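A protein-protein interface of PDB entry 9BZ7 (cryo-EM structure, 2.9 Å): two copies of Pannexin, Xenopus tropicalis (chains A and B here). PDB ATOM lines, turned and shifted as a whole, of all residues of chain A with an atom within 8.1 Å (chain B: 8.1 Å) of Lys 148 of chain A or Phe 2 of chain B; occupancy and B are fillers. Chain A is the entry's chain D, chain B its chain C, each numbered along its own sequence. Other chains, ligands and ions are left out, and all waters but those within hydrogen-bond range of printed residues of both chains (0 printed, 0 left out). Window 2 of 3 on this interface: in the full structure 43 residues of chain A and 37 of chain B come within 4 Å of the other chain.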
ATOM      1  N   TYR A 140     -18.679 -24.386   6.249  1.00  0.00           N
ATOM      2  CA  TYR A 140     -18.338 -24.371   7.667  1.00  0.00           C
ATOM      3  C   TYR A 140     -18.425 -25.764   8.270  1.00  0.00           C
ATOM      4  O   TYR A 140     -17.549 -26.170   9.041  1.00  0.00           O
ATOM      5  CB  TYR A 140     -19.249 -23.415   8.433  1.00  0.00           C
ATOM      6  CG  TYR A 140     -19.332 -23.745   9.907  1.00  0.00           C
ATOM      7  CD1 TYR A 140     -18.297 -23.411  10.771  1.00  0.00           C
ATOM      8  CD2 TYR A 140     -20.438 -24.401  10.433  1.00  0.00           C
ATOM      9  CE1 TYR A 140     -18.364 -23.711  12.118  1.00  0.00           C
ATOM     10  CE2 TYR A 140     -20.512 -24.706  11.779  1.00  0.00           C
ATOM     11  CZ  TYR A 140     -19.474 -24.358  12.616  1.00  0.00           C
ATOM     12  OH  TYR A 140     -19.544 -24.660  13.957  1.00  0.00           O
ATOM     13  N   ASN A 141     -19.486 -26.508   7.947  1.00  0.00           N
ATOM     14  CA  ASN A 141     -19.638 -27.850   8.495  1.00  0.00           C
ATOM     15  C   ASN A 141     -18.507 -28.759   8.029  1.00  0.00           C
ATOM     16  O   ASN A 141     -17.924 -29.504   8.826  1.00  0.00           O
ATOM     17  CB  ASN A 141     -20.999 -28.424   8.100  1.00  0.00           C
ATOM     18  CG  ASN A 141     -22.049 -28.206   9.170  1.00  0.00           C
ATOM     19  OD1 ASN A 141     -21.859 -27.410  10.089  1.00  0.00           O
ATOM     20  ND2 ASN A 141     -23.168 -28.910   9.053  1.00  0.00           N
ATOM     21  N   ARG A 142     -18.168 -28.693   6.738  1.00  0.00           N
ATOM     22  CA  ARG A 142     -17.081 -29.514   6.215  1.00  0.00           C
ATOM     23  C   ARG A 142     -15.756 -29.169   6.884  1.00  0.00           C
ATOM     24  O   ARG A 142     -14.987 -30.061   7.263  1.00  0.00           O
ATOM     25  CB  ARG A 142     -16.983 -29.340   4.700  1.00  0.00           C
ATOM     26  CG  ARG A 142     -17.709 -30.410   3.899  1.00  0.00           C
ATOM     27  CD  ARG A 142     -17.507 -30.337   2.372  1.00  0.00           C
ATOM     28  NE  ARG A 142     -17.466 -28.993   1.796  1.00  0.00           N
ATOM     29  CZ  ARG A 142     -16.400 -28.203   1.765  1.00  0.00           C
ATOM     30  NH1 ARG A 142     -15.223 -28.607   2.213  1.00  0.00           N
ATOM     31  NH2 ARG A 142     -16.515 -26.982   1.248  1.00  0.00           N
ATOM     32  N   ASP A 143     -15.475 -27.875   7.044  1.00  0.00           N
ATOM     33  CA  ASP A 143     -14.207 -27.460   7.637  1.00  0.00           C
ATOM     34  C   ASP A 143     -14.131 -27.852   9.108  1.00  0.00           C
ATOM     35  O   ASP A 143     -13.085 -28.310   9.585  1.00  0.00           O
ATOM     36  CB  ASP A 143     -14.017 -25.955   7.461  1.00  0.00           C
ATOM     37  CG  ASP A 143     -13.831 -25.561   6.009  1.00  0.00           C
ATOM     38  OD1 ASP A 143     -14.006 -26.430   5.129  1.00  0.00           O
ATOM     39  OD2 ASP A 143     -13.509 -24.384   5.743  1.00  0.00           O
ATOM     40  N   ILE A 144     -15.231 -27.687   9.846  1.00  0.00           N
ATOM     41  CA  ILE A 144     -15.221 -28.021  11.267  1.00  0.00           C
ATOM     42  C   ILE A 144     -15.176 -29.532  11.460  1.00  0.00           C
ATOM     43  O   ILE A 144     -14.723 -30.026  12.500  1.00  0.00           O
ATOM     44  CB  ILE A 144     -16.430 -27.383  11.980  1.00  0.00           C
ATOM     45  CG1 ILE A 144     -16.126 -27.177  13.465  1.00  0.00           C
ATOM     46  CG2 ILE A 144     -17.683 -28.226  11.802  1.00  0.00           C
ATOM     47  CD1 ILE A 144     -15.573 -25.806  13.792  1.00  0.00           C
ATOM     48  N   LYS A 145     -15.645 -30.291  10.467  1.00  0.00           N
ATOM     49  CA  LYS A 145     -15.505 -31.741  10.530  1.00  0.00           C
ATOM     50  C   LYS A 145     -14.077 -32.170  10.221  1.00  0.00           C
ATOM     51  O   LYS A 145     -13.558 -33.111  10.832  1.00  0.00           O
ATOM     52  CB  LYS A 145     -16.491 -32.407   9.569  1.00  0.00           C
ATOM     53  CG  LYS A 145     -16.523 -33.924   9.663  1.00  0.00           C
ATOM     54  CD  LYS A 145     -17.715 -34.499   8.916  1.00  0.00           C
ATOM     55  CE  LYS A 145     -17.753 -34.021   7.475  1.00  0.00           C
ATOM     56  NZ  LYS A 145     -18.977 -34.487   6.766  1.00  0.00           N
ATOM     57  N   ASP A 146     -13.426 -31.490   9.270  1.00  0.00           N
ATOM     58  CA  ASP A 146     -12.047 -31.829   8.931  1.00  0.00           C
ATOM     59  C   ASP A 146     -11.089 -31.544  10.081  1.00  0.00           C
ATOM     60  O   ASP A 146     -10.203 -32.359  10.363  1.00  0.00           O
ATOM     61  CB  ASP A 146     -11.612 -31.069   7.679  1.00  0.00           C
ATOM     62  CG  ASP A 146     -12.308 -31.564   6.425  1.00  0.00           C
ATOM     63  OD1 ASP A 146     -13.147 -32.484   6.532  1.00  0.00           O
ATOM     64  OD2 ASP A 146     -12.017 -31.033   5.333  1.00  0.00           O
ATOM     65  N   ILE A 147     -11.248 -30.400  10.756  1.00  0.00           N
ATOM     66  CA  ILE A 147     -10.376 -30.042  11.872  1.00  0.00           C
ATOM     67  C   ILE A 147     -10.675 -30.859  13.124  1.00  0.00           C
ATOM     68  O   ILE A 147      -9.816 -30.950  14.013  1.00  0.00           O
ATOM     69  CB  ILE A 147     -10.484 -28.527  12.161  1.00  0.00           C
ATOM     70  CG1 ILE A 147     -10.258 -27.726  10.878  1.00  0.00           C
ATOM     71  CG2 ILE A 147      -9.464 -28.084  13.200  1.00  0.00           C
ATOM     72  CD1 ILE A 147     -10.299 -26.227  11.079  1.00  0.00           C
ATOM     73  N   LYS A 148     -11.851 -31.477  13.204  1.00  0.00           N
ATOM     74  CA  LYS A 148     -12.270 -32.261  14.368  1.00  0.00           C
ATOM     75  C   LYS A 148     -12.283 -31.406  15.632  1.00  0.00           C
ATOM     76  O   LYS A 148     -12.578 -31.896  16.722  1.00  0.00           O
ATOM     77  CB  LYS A 148     -11.361 -33.479  14.571  1.00  0.00           C
ATOM     78  CG  LYS A 148     -11.069 -34.271  13.306  1.00  0.00           C
ATOM     79  CD  LYS A 148      -9.984 -35.308  13.556  1.00  0.00           C
ATOM     80  CE  LYS A 148      -9.599 -36.031  12.276  1.00  0.00           C
ATOM     81  NZ  LYS A 148      -8.499 -37.008  12.502  1.00  0.00           N
ATOM     82  N   VAL A 303     -11.524 -17.717   9.542  1.00  0.00           N
ATOM     83  CA  VAL A 303     -10.981 -18.644  10.531  1.00  0.00           C
ATOM     84  C   VAL A 303     -10.910 -20.048   9.946  1.00  0.00           C
ATOM     85  O   VAL A 303      -9.954 -20.796  10.193  1.00  0.00           O
ATOM     86  CB  VAL A 303     -11.825 -18.598  11.820  1.00  0.00           C
ATOM     87  CG1 VAL A 303     -11.704 -19.901  12.601  1.00  0.00           C
ATOM     88  CG2 VAL A 303     -11.411 -17.415  12.683  1.00  0.00           C
ATOM     89  N   LEU A 343     -15.963 -18.471  18.432  1.00  0.00           N
ATOM     90  CA  LEU A 343     -14.618 -18.975  18.167  1.00  0.00           C
ATOM     91  C   LEU A 343     -13.625 -17.833  17.976  1.00  0.00           C
ATOM     92  O   LEU A 343     -12.480 -17.916  18.435  1.00  0.00           O
ATOM     93  CB  LEU A 343     -14.633 -19.891  16.943  1.00  0.00           C
ATOM     94  CG  LEU A 343     -14.550 -21.398  17.208  1.00  0.00           C
ATOM     95  CD1 LEU A 343     -15.523 -21.822  18.301  1.00  0.00           C
ATOM     96  CD2 LEU A 343     -14.803 -22.184  15.931  1.00  0.00           C
ATOM     97  N   ILE A 346     -12.798 -16.487  21.248  1.00  0.00           N
ATOM     98  CA  ILE A 346     -11.908 -17.372  21.997  1.00  0.00           C
ATOM     99  C   ILE A 346     -10.465 -16.896  21.874  1.00  0.00           C
ATOM    100  O   ILE A 346      -9.729 -16.816  22.866  1.00  0.00           O
ATOM    101  CB  ILE A 346     -12.064 -18.825  21.515  1.00  0.00           C
ATOM    102  CG1 ILE A 346     -13.361 -19.433  22.049  1.00  0.00           C
ATOM    103  CG2 ILE A 346     -10.870 -19.668  21.941  1.00  0.00           C
ATOM    104  CD1 ILE A 346     -13.720 -20.752  21.407  1.00  0.00           C
ATOM    105  N   LYS A 347     -10.046 -16.560  20.659  1.00  0.00           N
ATOM    106  CA  LYS A 347      -8.687 -16.099  20.412  1.00  0.00           C
ATOM    107  C   LYS A 347      -8.581 -14.587  20.583  1.00  0.00           C
ATOM    108  O   LYS A 347      -9.059 -13.822  19.745  1.00  0.00           O
ATOM    109  CB  LYS A 347      -8.238 -16.502  19.005  1.00  0.00           C
ATOM    110  CG  LYS A 347      -8.273 -17.999  18.751  1.00  0.00           C
ATOM    111  CD  LYS A 347      -7.987 -18.319  17.294  1.00  0.00           C
ATOM    112  CE  LYS A 347      -8.056 -19.815  17.035  1.00  0.00           C
ATOM    113  NZ  LYS A 347      -7.823 -20.144  15.601  1.00  0.00           N
ATOM    114  N   VAL B   1     -14.234 -30.631  23.205  1.00  0.00           N
ATOM    115  CA  VAL B   1     -13.637 -30.873  21.898  1.00  0.00           C
ATOM    116  C   VAL B   1     -14.420 -30.137  20.816  1.00  0.00           C
ATOM    117  O   VAL B   1     -15.509 -29.621  21.068  1.00  0.00           O
ATOM    118  CB  VAL B   1     -13.567 -32.379  21.588  1.00  0.00           C
ATOM    119  N   PHE B   2     -13.857 -30.094  19.610  1.00  0.00           N
ATOM    120  CA  PHE B   2     -14.498 -29.422  18.479  1.00  0.00           C
ATOM    121  C   PHE B   2     -15.354 -30.410  17.683  1.00  0.00           C
ATOM    122  O   PHE B   2     -15.216 -30.573  16.471  1.00  0.00           O
ATOM    123  CB  PHE B   2     -13.448 -28.757  17.596  1.00  0.00           C
ATOM    124  CG  PHE B   2     -12.947 -27.441  18.125  1.00  0.00           C
ATOM    125  CD1 PHE B   2     -13.289 -27.010  19.396  1.00  0.00           C
ATOM    126  CD2 PHE B   2     -12.131 -26.635  17.348  1.00  0.00           C
ATOM    127  CE1 PHE B   2     -12.829 -25.800  19.881  1.00  0.00           C
ATOM    128  CE2 PHE B   2     -11.668 -25.424  17.827  1.00  0.00           C
ATOM    129  CZ  PHE B   2     -12.017 -25.006  19.096  1.00  0.00           C
ATOM    130  N   SER B   3     -16.255 -31.078  18.402  1.00  0.00           N
ATOM    131  CA  SER B   3     -17.154 -32.054  17.802  1.00  0.00           C
ATOM    132  C   SER B   3     -18.628 -31.750  18.020  1.00  0.00           C
ATOM    133  O   SER B   3     -19.468 -32.380  17.366  1.00  0.00           O
ATOM    134  CB  SER B   3     -16.855 -33.463  18.339  1.00  0.00           C
ATOM    135  OG  SER B   3     -17.900 -34.364  18.016  1.00  0.00           O
ATOM    136  N   ASP B   4     -18.972 -30.819  18.907  1.00  0.00           N
ATOM    137  CA  ASP B   4     -20.356 -30.461  19.180  1.00  0.00           C
ATOM    138  C   ASP B   4     -20.838 -29.286  18.338  1.00  0.00           C
ATOM    139  O   ASP B   4     -21.963 -28.817  18.536  1.00  0.00           O
ATOM    140  CB  ASP B   4     -20.527 -30.136  20.666  1.00  0.00           C
ATOM    141  CG  ASP B   4     -20.036 -31.251  21.567  1.00  0.00           C
ATOM    142  OD1 ASP B   4     -19.515 -32.257  21.041  1.00  0.00           O
ATOM    143  OD2 ASP B   4     -20.166 -31.119  22.802  1.00  0.00           O
ATOM    144  N   PHE B   5     -20.016 -28.803  17.410  1.00  0.00           N
ATOM    145  CA  PHE B   5     -20.336 -27.626  16.615  1.00  0.00           C
ATOM    146  C   PHE B   5     -21.105 -27.955  15.340  1.00  0.00           C
ATOM    147  O   PHE B   5     -21.416 -27.040  14.571  1.00  0.00           O
ATOM    148  CB  PHE B   5     -19.052 -26.870  16.261  1.00  0.00           C
ATOM    149  CG  PHE B   5     -18.346 -26.284  17.451  1.00  0.00           C
ATOM    150  CD1 PHE B   5     -17.437 -27.037  18.174  1.00  0.00           C
ATOM    151  CD2 PHE B   5     -18.596 -24.981  17.848  1.00  0.00           C
ATOM    152  CE1 PHE B   5     -16.788 -26.503  19.270  1.00  0.00           C
ATOM    153  CE2 PHE B   5     -17.948 -24.440  18.944  1.00  0.00           C
ATOM    154  CZ  PHE B   5     -17.044 -25.202  19.655  1.00  0.00           C
ATOM    155  N   LEU B   6     -21.414 -29.227  15.097  1.00  0.00           N
ATOM    156  CA  LEU B   6     -22.175 -29.599  13.914  1.00  0.00           C
ATOM    157  C   LEU B   6     -23.610 -29.093  14.016  1.00  0.00           C
ATOM    158  O   LEU B   6     -24.189 -29.010  15.102  1.00  0.00           O
ATOM    159  CB  LEU B   6     -22.165 -31.116  13.726  1.00  0.00           C
ATOM    160  CG  LEU B   6     -21.021 -31.702  12.894  1.00  0.00           C
ATOM    161  CD1 LEU B   6     -20.870 -30.950  11.579  1.00  0.00           C
ATOM    162  CD2 LEU B   6     -19.714 -31.694  13.675  1.00  0.00           C
ATOM    163  N   TYR B 185     -17.383 -27.468  26.847  1.00  0.00           N
ATOM    164  CA  TYR B 185     -17.006 -26.074  26.647  1.00  0.00           C
ATOM    165  C   TYR B 185     -18.198 -25.145  26.854  1.00  0.00           C
ATOM    166  O   TYR B 185     -19.278 -25.384  26.315  1.00  0.00           O
ATOM    167  CB  TYR B 185     -16.422 -25.870  25.248  1.00  0.00           C
ATOM    168  CG  TYR B 185     -15.468 -24.702  25.150  1.00  0.00           C
ATOM    169  CD1 TYR B 185     -14.355 -24.617  25.978  1.00  0.00           C
ATOM    170  CD2 TYR B 185     -15.685 -23.678  24.238  1.00  0.00           C
ATOM    171  CE1 TYR B 185     -13.480 -23.549  25.892  1.00  0.00           C
ATOM    172  CE2 TYR B 185     -14.819 -22.607  24.148  1.00  0.00           C
ATOM    173  CZ  TYR B 185     -13.718 -22.547  24.976  1.00  0.00           C
ATOM    174  OH  TYR B 185     -12.853 -21.481  24.886  1.00  0.00           O
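Of the 13 printed residues of chain A, 5 touch a printed residue of chain B. Hydrophobic or aromatic side chains of chain A that line the printed part of chain B: Tyr 140, Leu 343 and Ile 346. Printed residues of chain B that touch a printed residue of chain A: Phe 2, Phe 5, Leu 6 and Tyr 185. Hydrophobic or aromatic side chains of chain B that line the printed part of chain A: Phe 2, Phe 5, Leu 6 and Tyr 185. Among the printed residues, 5 pairs touch across the chains.
Of the printed residues of chain B, Asn 141 of chain A touches Leu 6 (3.8 Å). Lys 148 of chain A touches just one residue of chain B: Phe 2 (3.0 Å). Printed residues of chain B within 4 Å of Leu 343 of chain A: Phe 5. No residue of chain A comes within 4 Å of Val 1 of chain B. Of chain A, only Lys 148 comes within 4 Å of Phe 2 of chain B. Of the printed residues of chain A, Phe 5 of chain B touches Tyr 140 and Leu 343. Printed residues of chain A within 4 Å of Tyr 185 of chain B: Ile 346 (3.5 Å). The nearest residue of chain A that does not touch Phe 2 of chain B is Ile 144 of chain A (4.04 Å).
Asn 141 of chain A touches Leu 6 of chain B. Leu 343 of chain A touches Phe 5 of chain B (CD1 to CE2, 3.6 Å). CD1 of Ile 346 of chain A touches CE2 of Tyr 185 of chain B, at 3.5 Å.
O of Phe 5 of chain B lies within hydrogen-bond range of OH of Tyr 140 of chain A, at 3.1 Å. O of Lys 148 of chain A lies close to O of Phe 2 of chain B, at 3.0 Å.
No position is printed for both chains.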
